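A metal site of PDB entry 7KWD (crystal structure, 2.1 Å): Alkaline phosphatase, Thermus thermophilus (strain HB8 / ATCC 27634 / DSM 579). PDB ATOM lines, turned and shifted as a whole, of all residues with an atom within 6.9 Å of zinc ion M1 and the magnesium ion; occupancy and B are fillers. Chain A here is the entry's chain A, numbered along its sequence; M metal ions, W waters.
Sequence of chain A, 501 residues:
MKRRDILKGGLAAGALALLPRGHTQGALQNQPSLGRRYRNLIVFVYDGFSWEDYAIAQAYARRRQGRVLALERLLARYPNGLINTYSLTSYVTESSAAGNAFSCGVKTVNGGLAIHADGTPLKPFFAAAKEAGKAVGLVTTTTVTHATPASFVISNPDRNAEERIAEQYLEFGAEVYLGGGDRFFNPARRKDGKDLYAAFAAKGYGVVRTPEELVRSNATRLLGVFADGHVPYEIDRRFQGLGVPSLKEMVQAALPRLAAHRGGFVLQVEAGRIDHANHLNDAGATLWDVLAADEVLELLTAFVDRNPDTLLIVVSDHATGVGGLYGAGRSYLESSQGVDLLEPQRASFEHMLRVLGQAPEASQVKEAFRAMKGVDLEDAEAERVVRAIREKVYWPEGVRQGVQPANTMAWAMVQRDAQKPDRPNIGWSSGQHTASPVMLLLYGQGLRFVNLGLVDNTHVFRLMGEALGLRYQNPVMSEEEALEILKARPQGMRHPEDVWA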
ATOM      1  N   VAL A  45       9.080  24.203  -5.513  1.00  0.00           N
ATOM      2  CA  VAL A  45       8.021  25.209  -5.684  1.00  0.00           C
ATOM      3  C   VAL A  45       6.708  24.497  -5.973  1.00  0.00           C
ATOM      4  O   VAL A  45       6.610  23.720  -6.932  1.00  0.00           O
ATOM      5  CB  VAL A  45       8.347  26.189  -6.807  1.00  0.00           C
ATOM      6  CG1 VAL A  45       7.207  27.196  -6.962  1.00  0.00           C
ATOM      7  CG2 VAL A  45       9.677  26.860  -6.543  1.00  0.00           C
ATOM      8  N   TYR A  46       5.696  24.779  -5.163  1.00  0.00           N
ATOM      9  CA  TYR A  46       4.301  24.435  -5.437  1.00  0.00           C
ATOM     10  C   TYR A  46       3.664  25.642  -6.111  1.00  0.00           C
ATOM     11  O   TYR A  46       3.269  26.602  -5.462  1.00  0.00           O
ATOM     12  CB  TYR A  46       3.584  24.090  -4.141  1.00  0.00           C
ATOM     13  CG  TYR A  46       3.798  22.709  -3.543  1.00  0.00           C
ATOM     14  CD1 TYR A  46       5.054  22.264  -3.162  1.00  0.00           C
ATOM     15  CD2 TYR A  46       2.711  21.883  -3.255  1.00  0.00           C
ATOM     16  CE1 TYR A  46       5.224  21.025  -2.565  1.00  0.00           C
ATOM     17  CE2 TYR A  46       2.869  20.650  -2.655  1.00  0.00           C
ATOM     18  CZ  TYR A  46       4.126  20.229  -2.310  1.00  0.00           C
ATOM     19  OH  TYR A  46       4.295  18.990  -1.738  1.00  0.00           O
ATOM     20  N   ASP A  47       3.574  25.631  -7.444  1.00  0.00           N
ATOM     21  CA  ASP A  47       3.086  26.795  -8.160  1.00  0.00           C
ATOM     22  C   ASP A  47       1.580  26.929  -8.005  1.00  0.00           C
ATOM     23  O   ASP A  47       0.836  25.996  -8.276  1.00  0.00           O
ATOM     24  CB  ASP A  47       3.464  26.700  -9.641  1.00  0.00           C
ATOM     25  CG  ASP A  47       3.452  28.032 -10.293  1.00  0.00           C
ATOM     26  OD1 ASP A  47       2.386  28.673 -10.211  1.00  0.00           O
ATOM     27  OD2 ASP A  47       4.500  28.453 -10.856  1.00  0.00           O
ATOM     28  N   GLY A  48       1.132  28.105  -7.571  1.00  0.00           N
ATOM     29  CA  GLY A  48      -0.297  28.375  -7.455  1.00  0.00           C
ATOM     30  C   GLY A  48      -1.006  27.724  -6.287  1.00  0.00           C
ATOM     31  O   GLY A  48      -2.248  27.738  -6.229  1.00  0.00           O
ATOM     32  N   THR A  93       0.632  38.847  -7.965  1.00  0.00           N
ATOM     33  CA  THR A  93       1.794  38.621  -8.813  1.00  0.00           C
ATOM     34  C   THR A  93       1.423  37.612  -9.891  1.00  0.00           C
ATOM     35  O   THR A  93       0.437  36.899  -9.798  1.00  0.00           O
ATOM     36  CB  THR A  93       2.942  38.072  -7.972  1.00  0.00           C
ATOM     37  OG1 THR A  93       4.176  38.052  -8.688  1.00  0.00           O
ATOM     38  CG2 THR A  93       2.619  36.656  -7.538  1.00  0.00           C
ATOM     39  N   GLU A  94       2.276  37.503 -10.895  1.00  0.00           N
ATOM     40  CA  GLU A  94       2.298  36.241 -11.649  1.00  0.00           C
ATOM     41  C   GLU A  94       3.680  35.606 -11.480  1.00  0.00           C
ATOM     42  O   GLU A  94       4.507  36.047 -10.675  1.00  0.00           O
ATOM     43  CB  GLU A  94       1.859  36.446 -13.102  1.00  0.00           C
ATOM     44  CG  GLU A  94       2.521  37.593 -13.795  1.00  0.00           C
ATOM     45  CD  GLU A  94       4.036  37.351 -13.910  1.00  0.00           C
ATOM     46  OE1 GLU A  94       4.771  37.847 -13.021  1.00  0.00           O
ATOM     47  OE2 GLU A  94       4.489  36.658 -14.865  1.00  0.00           O
ATOM     48  N   SER A  95       3.912  34.547 -12.261  1.00  0.00           N
ATOM     49  CA  SER A  95       4.965  33.605 -11.932  1.00  0.00           C
ATOM     50  C   SER A  95       6.366  34.183 -12.138  1.00  0.00           C
ATOM     51  O   SER A  95       7.292  33.840 -11.387  1.00  0.00           O
ATOM     52  CB  SER A  95       4.797  32.349 -12.761  1.00  0.00           C
ATOM     53  OG  SER A  95       4.075  31.387 -12.069  1.00  0.00           O
ATOM     54  N   SER A  96       6.575  35.026 -13.166  1.00  0.00           N
ATOM     55  CA  SER A  96       7.929  35.535 -13.408  1.00  0.00           C
ATOM     56  C   SER A  96       8.363  36.485 -12.301  1.00  0.00           C
ATOM     57  O   SER A  96       9.478  36.375 -11.775  1.00  0.00           O
ATOM     58  CB  SER A  96       8.045  36.244 -14.765  1.00  0.00           C
ATOM     59  OG  SER A  96       7.067  37.248 -14.903  1.00  0.00           O
ATOM     60  N   ALA A  98       7.172  36.495  -9.301  1.00  0.00           N
ATOM     61  CA  ALA A  98       7.304  35.703  -8.076  1.00  0.00           C
ATOM     62  C   ALA A  98       8.616  34.949  -8.084  1.00  0.00           C
ATOM     63  O   ALA A  98       9.366  34.973  -7.102  1.00  0.00           O
ATOM     64  CB  ALA A  98       6.129  34.744  -7.967  1.00  0.00           C
ATOM     65  N   THR A 140      10.505  20.081 -13.867  1.00  0.00           N
ATOM     66  CA  THR A 140       9.167  20.645 -13.712  1.00  0.00           C
ATOM     67  C   THR A 140       8.140  19.896 -14.549  1.00  0.00           C
ATOM     68  O   THR A 140       8.493  19.182 -15.477  1.00  0.00           O
ATOM     69  CB  THR A 140       9.155  22.114 -14.125  1.00  0.00           C
ATOM     70  OG1 THR A 140       7.823  22.634 -14.091  1.00  0.00           O
ATOM     71  CG2 THR A 140       9.715  22.276 -15.541  1.00  0.00           C
ATOM     72  N   THR A 142       5.738  21.838 -15.946  1.00  0.00           N
ATOM     73  CA  THR A 142       5.475  22.761 -17.039  1.00  0.00           C
ATOM     74  C   THR A 142       6.472  22.507 -18.168  1.00  0.00           C
ATOM     75  O   THR A 142       7.383  21.675 -18.047  1.00  0.00           O
ATOM     76  CB  THR A 142       5.567  24.211 -16.566  1.00  0.00           C
ATOM     77  OG1 THR A 142       6.926  24.495 -16.197  1.00  0.00           O
ATOM     78  CG2 THR A 142       4.646  24.482 -15.358  1.00  0.00           C
ATOM     79  N   HIS A 146       9.557  27.311 -18.890  1.00  0.00           N
ATOM     80  CA  HIS A 146       8.543  28.162 -18.295  1.00  0.00           C
ATOM     81  C   HIS A 146       9.144  29.061 -17.218  1.00  0.00           C
ATOM     82  O   HIS A 146      10.324  28.966 -16.867  1.00  0.00           O
ATOM     83  CB  HIS A 146       7.413  27.297 -17.757  1.00  0.00           C
ATOM     84  CG  HIS A 146       6.066  27.940 -17.803  1.00  0.00           C
ATOM     85  ND1 HIS A 146       5.311  28.148 -16.675  1.00  0.00           N
ATOM     86  CD2 HIS A 146       5.316  28.372 -18.855  1.00  0.00           C
ATOM     87  CE1 HIS A 146       4.160  28.696 -17.014  1.00  0.00           C
ATOM     88  NE2 HIS A 146       4.136  28.854 -18.331  1.00  0.00           N
ATOM     89  N   ALA A 147       8.316  29.986 -16.733  1.00  0.00           N
ATOM     90  CA  ALA A 147       8.824  31.119 -15.960  1.00  0.00           C
ATOM     91  C   ALA A 147       9.520  30.678 -14.687  1.00  0.00           C
ATOM     92  O   ALA A 147      10.571  31.236 -14.333  1.00  0.00           O
ATOM     93  CB  ALA A 147       7.680  32.061 -15.603  1.00  0.00           C
ATOM     94  N   THR A 148       8.983  29.685 -13.987  1.00  0.00           N
ATOM     95  CA  THR A 148       9.513  29.406 -12.656  1.00  0.00           C
ATOM     96  C   THR A 148      10.915  28.838 -12.729  1.00  0.00           C
ATOM     97  O   THR A 148      11.813  29.362 -12.054  1.00  0.00           O
ATOM     98  CB  THR A 148       8.555  28.480 -11.910  1.00  0.00           C
ATOM     99  OG1 THR A 148       7.287  29.127 -11.751  1.00  0.00           O
ATOM    100  CG2 THR A 148       9.131  28.150 -10.560  1.00  0.00           C
ATOM    101  N   PRO A 149      11.194  27.808 -13.524  1.00  0.00           N
ATOM    102  CA  PRO A 149      12.592  27.371 -13.681  1.00  0.00           C
ATOM    103  C   PRO A 149      13.442  28.422 -14.340  1.00  0.00           C
ATOM    104  O   PRO A 149      14.598  28.657 -13.921  1.00  0.00           O
ATOM    105  CB  PRO A 149      12.470  26.102 -14.552  1.00  0.00           C
ATOM    106  CG  PRO A 149      11.106  26.154 -15.159  1.00  0.00           C
ATOM    107  CD  PRO A 149      10.233  26.908 -14.171  1.00  0.00           C
ATOM    108  N   ARG A 159       8.819  36.528 -20.763  1.00  0.00           N
ATOM    109  CA  ARG A 159       8.751  35.162 -20.268  1.00  0.00           C
ATOM    110  C   ARG A 159       8.259  34.212 -21.344  1.00  0.00           C
ATOM    111  O   ARG A 159       8.601  33.032 -21.336  1.00  0.00           O
ATOM    112  CB  ARG A 159       7.835  35.071 -19.032  1.00  0.00           C
ATOM    113  CG  ARG A 159       6.406  35.580 -19.215  1.00  0.00           C
ATOM    114  CD  ARG A 159       5.487  35.235 -18.039  1.00  0.00           C
ATOM    115  NE  ARG A 159       5.270  33.793 -17.839  1.00  0.00           N
ATOM    116  CZ  ARG A 159       4.529  33.278 -16.862  1.00  0.00           C
ATOM    117  NH1 ARG A 159       4.337  31.967 -16.762  1.00  0.00           N
ATOM    118  NH2 ARG A 159       3.958  34.103 -15.975  1.00  0.00           N
ATOM    119  N   GLN A 268      15.947  22.979  -8.582  1.00  0.00           N
ATOM    120  CA  GLN A 268      14.578  23.417  -8.465  1.00  0.00           C
ATOM    121  C   GLN A 268      13.676  22.276  -8.955  1.00  0.00           C
ATOM    122  O   GLN A 268      13.889  21.734 -10.052  1.00  0.00           O
ATOM    123  CB  GLN A 268      14.289  24.688  -9.269  1.00  0.00           C
ATOM    124  CG  GLN A 268      12.874  25.234  -9.009  1.00  0.00           C
ATOM    125  CD  GLN A 268      12.393  26.263 -10.021  1.00  0.00           C
ATOM    126  OE1 GLN A 268      11.655  25.953 -10.943  1.00  0.00           O
ATOM    127  NE2 GLN A 268      12.761  27.522  -9.799  1.00  0.00           N
ATOM    128  N   GLU A 270       9.631  21.766  -9.610  1.00  0.00           N
ATOM    129  CA  GLU A 270       8.401  22.544  -9.702  1.00  0.00           C
ATOM    130  C   GLU A 270       7.200  21.636  -9.930  1.00  0.00           C
ATOM    131  O   GLU A 270       7.155  20.895 -10.923  1.00  0.00           O
ATOM    132  CB  GLU A 270       8.434  23.591 -10.812  1.00  0.00           C
ATOM    133  CG  GLU A 270       7.327  24.656 -10.535  1.00  0.00           C
ATOM    134  CD  GLU A 270       6.929  25.388 -11.768  1.00  0.00           C
ATOM    135  OE1 GLU A 270       7.438  25.026 -12.855  1.00  0.00           O
ATOM    136  OE2 GLU A 270       6.132  26.320 -11.630  1.00  0.00           O
ATOM    137  N   ALA A 271       6.248  21.693  -9.010  1.00  0.00           N
ATOM    138  CA  ALA A 271       4.914  21.162  -9.235  1.00  0.00           C
ATOM    139  C   ALA A 271       4.143  22.311  -9.847  1.00  0.00           C
ATOM    140  O   ALA A 271       3.392  23.029  -9.191  1.00  0.00           O
ATOM    141  CB  ALA A 271       4.282  20.661  -7.945  1.00  0.00           C
ATOM    142  N   GLY A 272       4.385  22.515 -11.156  1.00  0.00           N
ATOM    143  CA  GLY A 272       3.967  23.731 -11.796  1.00  0.00           C
ATOM    144  C   GLY A 272       2.561  23.765 -12.298  1.00  0.00           C
ATOM    145  O   GLY A 272       2.105  24.826 -12.761  1.00  0.00           O
ATOM    146  N   ARG A 273       1.835  22.641 -12.255  1.00  0.00           N
ATOM    147  CA  ARG A 273       0.499  22.621 -12.833  1.00  0.00           C
ATOM    148  C   ARG A 273      -0.593  22.611 -11.782  1.00  0.00           C
ATOM    149  O   ARG A 273      -1.792  22.600 -12.126  1.00  0.00           O
ATOM    150  CB  ARG A 273       0.361  21.419 -13.786  1.00  0.00           C
ATOM    151  CG  ARG A 273       1.476  21.395 -14.859  1.00  0.00           C
ATOM    152  CD  ARG A 273       1.054  20.803 -16.216  1.00  0.00           C
ATOM    153  NE  ARG A 273       0.072  21.673 -16.866  1.00  0.00           N
ATOM    154  CZ  ARG A 273      -0.800  21.266 -17.777  1.00  0.00           C
ATOM    155  NH1 ARG A 273      -0.822  19.995 -18.169  1.00  0.00           N
ATOM    156  NH2 ARG A 273      -1.646  22.142 -18.279  1.00  0.00           N
ATOM    157  N   ASP A 275      -1.021  25.342 -10.197  1.00  0.00           N
ATOM    158  CA  ASP A 275      -1.508  26.625 -10.712  1.00  0.00           C
ATOM    159  C   ASP A 275      -2.480  26.427 -11.859  1.00  0.00           C
ATOM    160  O   ASP A 275      -3.605  26.937 -11.836  1.00  0.00           O
ATOM    161  CB  ASP A 275      -0.298  27.470 -11.144  1.00  0.00           C
ATOM    162  CG  ASP A 275      -0.663  28.834 -11.630  1.00  0.00           C
ATOM    163  OD1 ASP A 275      -1.258  29.599 -10.823  1.00  0.00           O
ATOM    164  OD2 ASP A 275      -0.340  29.144 -12.803  1.00  0.00           O
ATOM    165  N   HIS A 276      -2.098  25.631 -12.856  1.00  0.00           N
ATOM    166  CA  HIS A 276      -2.913  25.475 -14.049  1.00  0.00           C
ATOM    167  C   HIS A 276      -4.268  24.871 -13.726  1.00  0.00           C
ATOM    168  O   HIS A 276      -5.298  25.324 -14.215  1.00  0.00           O
ATOM    169  CB  HIS A 276      -2.191  24.598 -15.076  1.00  0.00           C
ATOM    170  CG  HIS A 276      -0.898  25.195 -15.532  1.00  0.00           C
ATOM    171  ND1 HIS A 276      -0.014  24.510 -16.324  1.00  0.00           N
ATOM    172  CD2 HIS A 276      -0.323  26.394 -15.287  1.00  0.00           C
ATOM    173  CE1 HIS A 276       1.044  25.264 -16.574  1.00  0.00           C
ATOM    174  NE2 HIS A 276       0.882  26.407 -15.948  1.00  0.00           N
ATOM    175  N   ASP A 317       4.609  29.794  -4.748  1.00  0.00           N
ATOM    176  CA  ASP A 317       4.942  31.123  -5.287  1.00  0.00           C
ATOM    177  C   ASP A 317       3.801  32.120  -5.222  1.00  0.00           C
ATOM    178  O   ASP A 317       4.049  33.330  -5.285  1.00  0.00           O
ATOM    179  CB  ASP A 317       5.486  31.023  -6.710  1.00  0.00           C
ATOM    180  CG  ASP A 317       4.465  30.601  -7.716  1.00  0.00           C
ATOM    181  OD1 ASP A 317       3.454  29.934  -7.369  1.00  0.00           O
ATOM    182  OD2 ASP A 317       4.690  30.912  -8.898  1.00  0.00           O
ATOM    183  N   HIS A 318       2.564  31.650  -5.104  1.00  0.00           N
ATOM    184  CA  HIS A 318       1.378  32.463  -4.880  1.00  0.00           C
ATOM    185  C   HIS A 318       0.187  31.495  -4.869  1.00  0.00           C
ATOM    186  O   HIS A 318       0.284  30.354  -5.344  1.00  0.00           O
ATOM    187  CB  HIS A 318       1.140  33.513  -5.975  1.00  0.00           C
ATOM    188  CG  HIS A 318       1.139  32.894  -7.327  1.00  0.00           C
ATOM    189  ND1 HIS A 318       0.053  32.216  -7.834  1.00  0.00           N
ATOM    190  CD2 HIS A 318       2.130  32.743  -8.222  1.00  0.00           C
ATOM    191  CE1 HIS A 318       0.365  31.712  -9.007  1.00  0.00           C
ATOM    192  NE2 HIS A 318       1.613  32.032  -9.270  1.00  0.00           N
ATOM    193  N   THR A 320      -3.704  30.552  -6.192  1.00  0.00           N
ATOM    194  CA  THR A 320      -4.486  30.667  -7.414  1.00  0.00           C
ATOM    195  C   THR A 320      -5.870  30.068  -7.221  1.00  0.00           C
ATOM    196  O   THR A 320      -6.004  28.957  -6.691  1.00  0.00           O
ATOM    197  CB  THR A 320      -3.778  30.002  -8.591  1.00  0.00           C
ATOM    198  OG1 THR A 320      -2.543  30.666  -8.778  1.00  0.00           O
ATOM    199  CG2 THR A 320      -4.617  30.099  -9.892  1.00  0.00           C
ATOM    200  N   HIS A 433      -4.761  34.186 -10.223  1.00  0.00           N
ATOM    201  CA  HIS A 433      -4.011  34.255  -8.968  1.00  0.00           C
ATOM    202  C   HIS A 433      -4.709  35.154  -7.961  1.00  0.00           C
ATOM    203  O   HIS A 433      -5.480  36.051  -8.322  1.00  0.00           O
ATOM    204  CB  HIS A 433      -2.605  34.811  -9.171  1.00  0.00           C
ATOM    205  CG  HIS A 433      -1.829  34.096 -10.203  1.00  0.00           C
ATOM    206  ND1 HIS A 433      -0.590  34.515 -10.630  1.00  0.00           N
ATOM    207  CD2 HIS A 433      -2.111  32.971 -10.925  1.00  0.00           C
ATOM    208  CE1 HIS A 433      -0.140  33.694 -11.566  1.00  0.00           C
ATOM    209  NE2 HIS A 433      -1.047  32.767 -11.769  1.00  0.00           N
HETATM  210 ZN    ZN M   1       3.092  30.758 -10.371  1.00  0.00          ZN
HETATM  211 MG    MG M   2       5.474  27.920 -12.700  1.00  0.00          MG
HETATM  212 ZN    ZN M   3      -0.930  31.018 -13.075  1.00  0.00          ZN
HETATM  213  O   HOH W   1       4.965  29.475 -13.762  1.00  0.00           O
HETATM  214  O   HOH W   2       6.788  27.471 -14.308  1.00  0.00           O
HETATM  215  O   HOH W   3       3.444  26.970 -13.327  1.00  0.00           O
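Water W2 lies within hydrogen-bond range of a ring nitrogen (ND1) of His 146 (2.9 Å), the side-chain carboxylate of Glu 270 (2.9 Å) and the backbone NH of Thr 148 (3.1 Å).
Residues that only touch the magnesium ion: His 146 (3.98 Å).
Five residues have an atom within 4 Å of the magnesium ion: Asp 47, Ser 95, His 146, Thr 148 and Glu 270.
The side-chain hydroxyl (OG1) of Thr 142 sits at hydrogen-bond distance from the side-chain carboxylate (OE1) of Glu 270.
The side-chain hydroxyl (OG1) of Thr 140 sits at hydrogen-bond distance from the side-chain carboxylate (OE1) of Glu 270.
The backbone carbonyl oxygen (O) of Asp 47 lies within hydrogen-bond range of the backbone NH (N) of Asp 275 (2.8 Å).
The backbone carbonyl oxygen of Ala 271 is in hydrogen-bond range of the backbone NH of Asp 47, 3.1 Å away.
OD1 of Asp 317 lies within hydrogen-bond range of N of Gly 48 (3.0 Å).
N of Gly 48 lies close to O of His 318, 3.3 Å away.
ND1 of His 318 lies close to OG1 of Thr 320 (3.2 Å).
O of Thr 148 is in hydrogen-bond range of NE2 of Gln 268 (3.1 Å).
Water W1 is bound to the magnesium ion.
OE2 of Glu 270 binds the magnesium ion, 2.0 Å away.
Water W2 is bound to the magnesium ion, 2.1 Å away.
The magnesium ion is bound by the side-chain carboxylate (OD2) of Asp 47 (2.2 Å).
Water W3 binds the magnesium ion.
The side-chain hydroxyl (OG1) of Thr 148 binds the magnesium ion (2.4 Å).
The magnesium ion has six donor atoms within binding distance.
OG of Ser 95 binds zinc ion M1, 2.1 Å away.
OD2 of Asp 317 is bound to zinc ion M1, at 2.2 Å.
Zinc ion M1 is bound by OD1 of Asp 47.
A ring nitrogen (NE2) of His 318 is bound to zinc ion M1 (2.2 Å).
Zinc ion M1 has four donor atoms within binding distance.
Slightly farther from zinc ion M1 lies the side-chain carboxylate (OD2) of Asp 47 (2.7 Å).
Along chain A the residues within 4 Å of zinc ion M1 span positions 47 to 318.
The nearest printed residue that does not touch zinc ion M1 is Gly 48 (4.3 Å).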
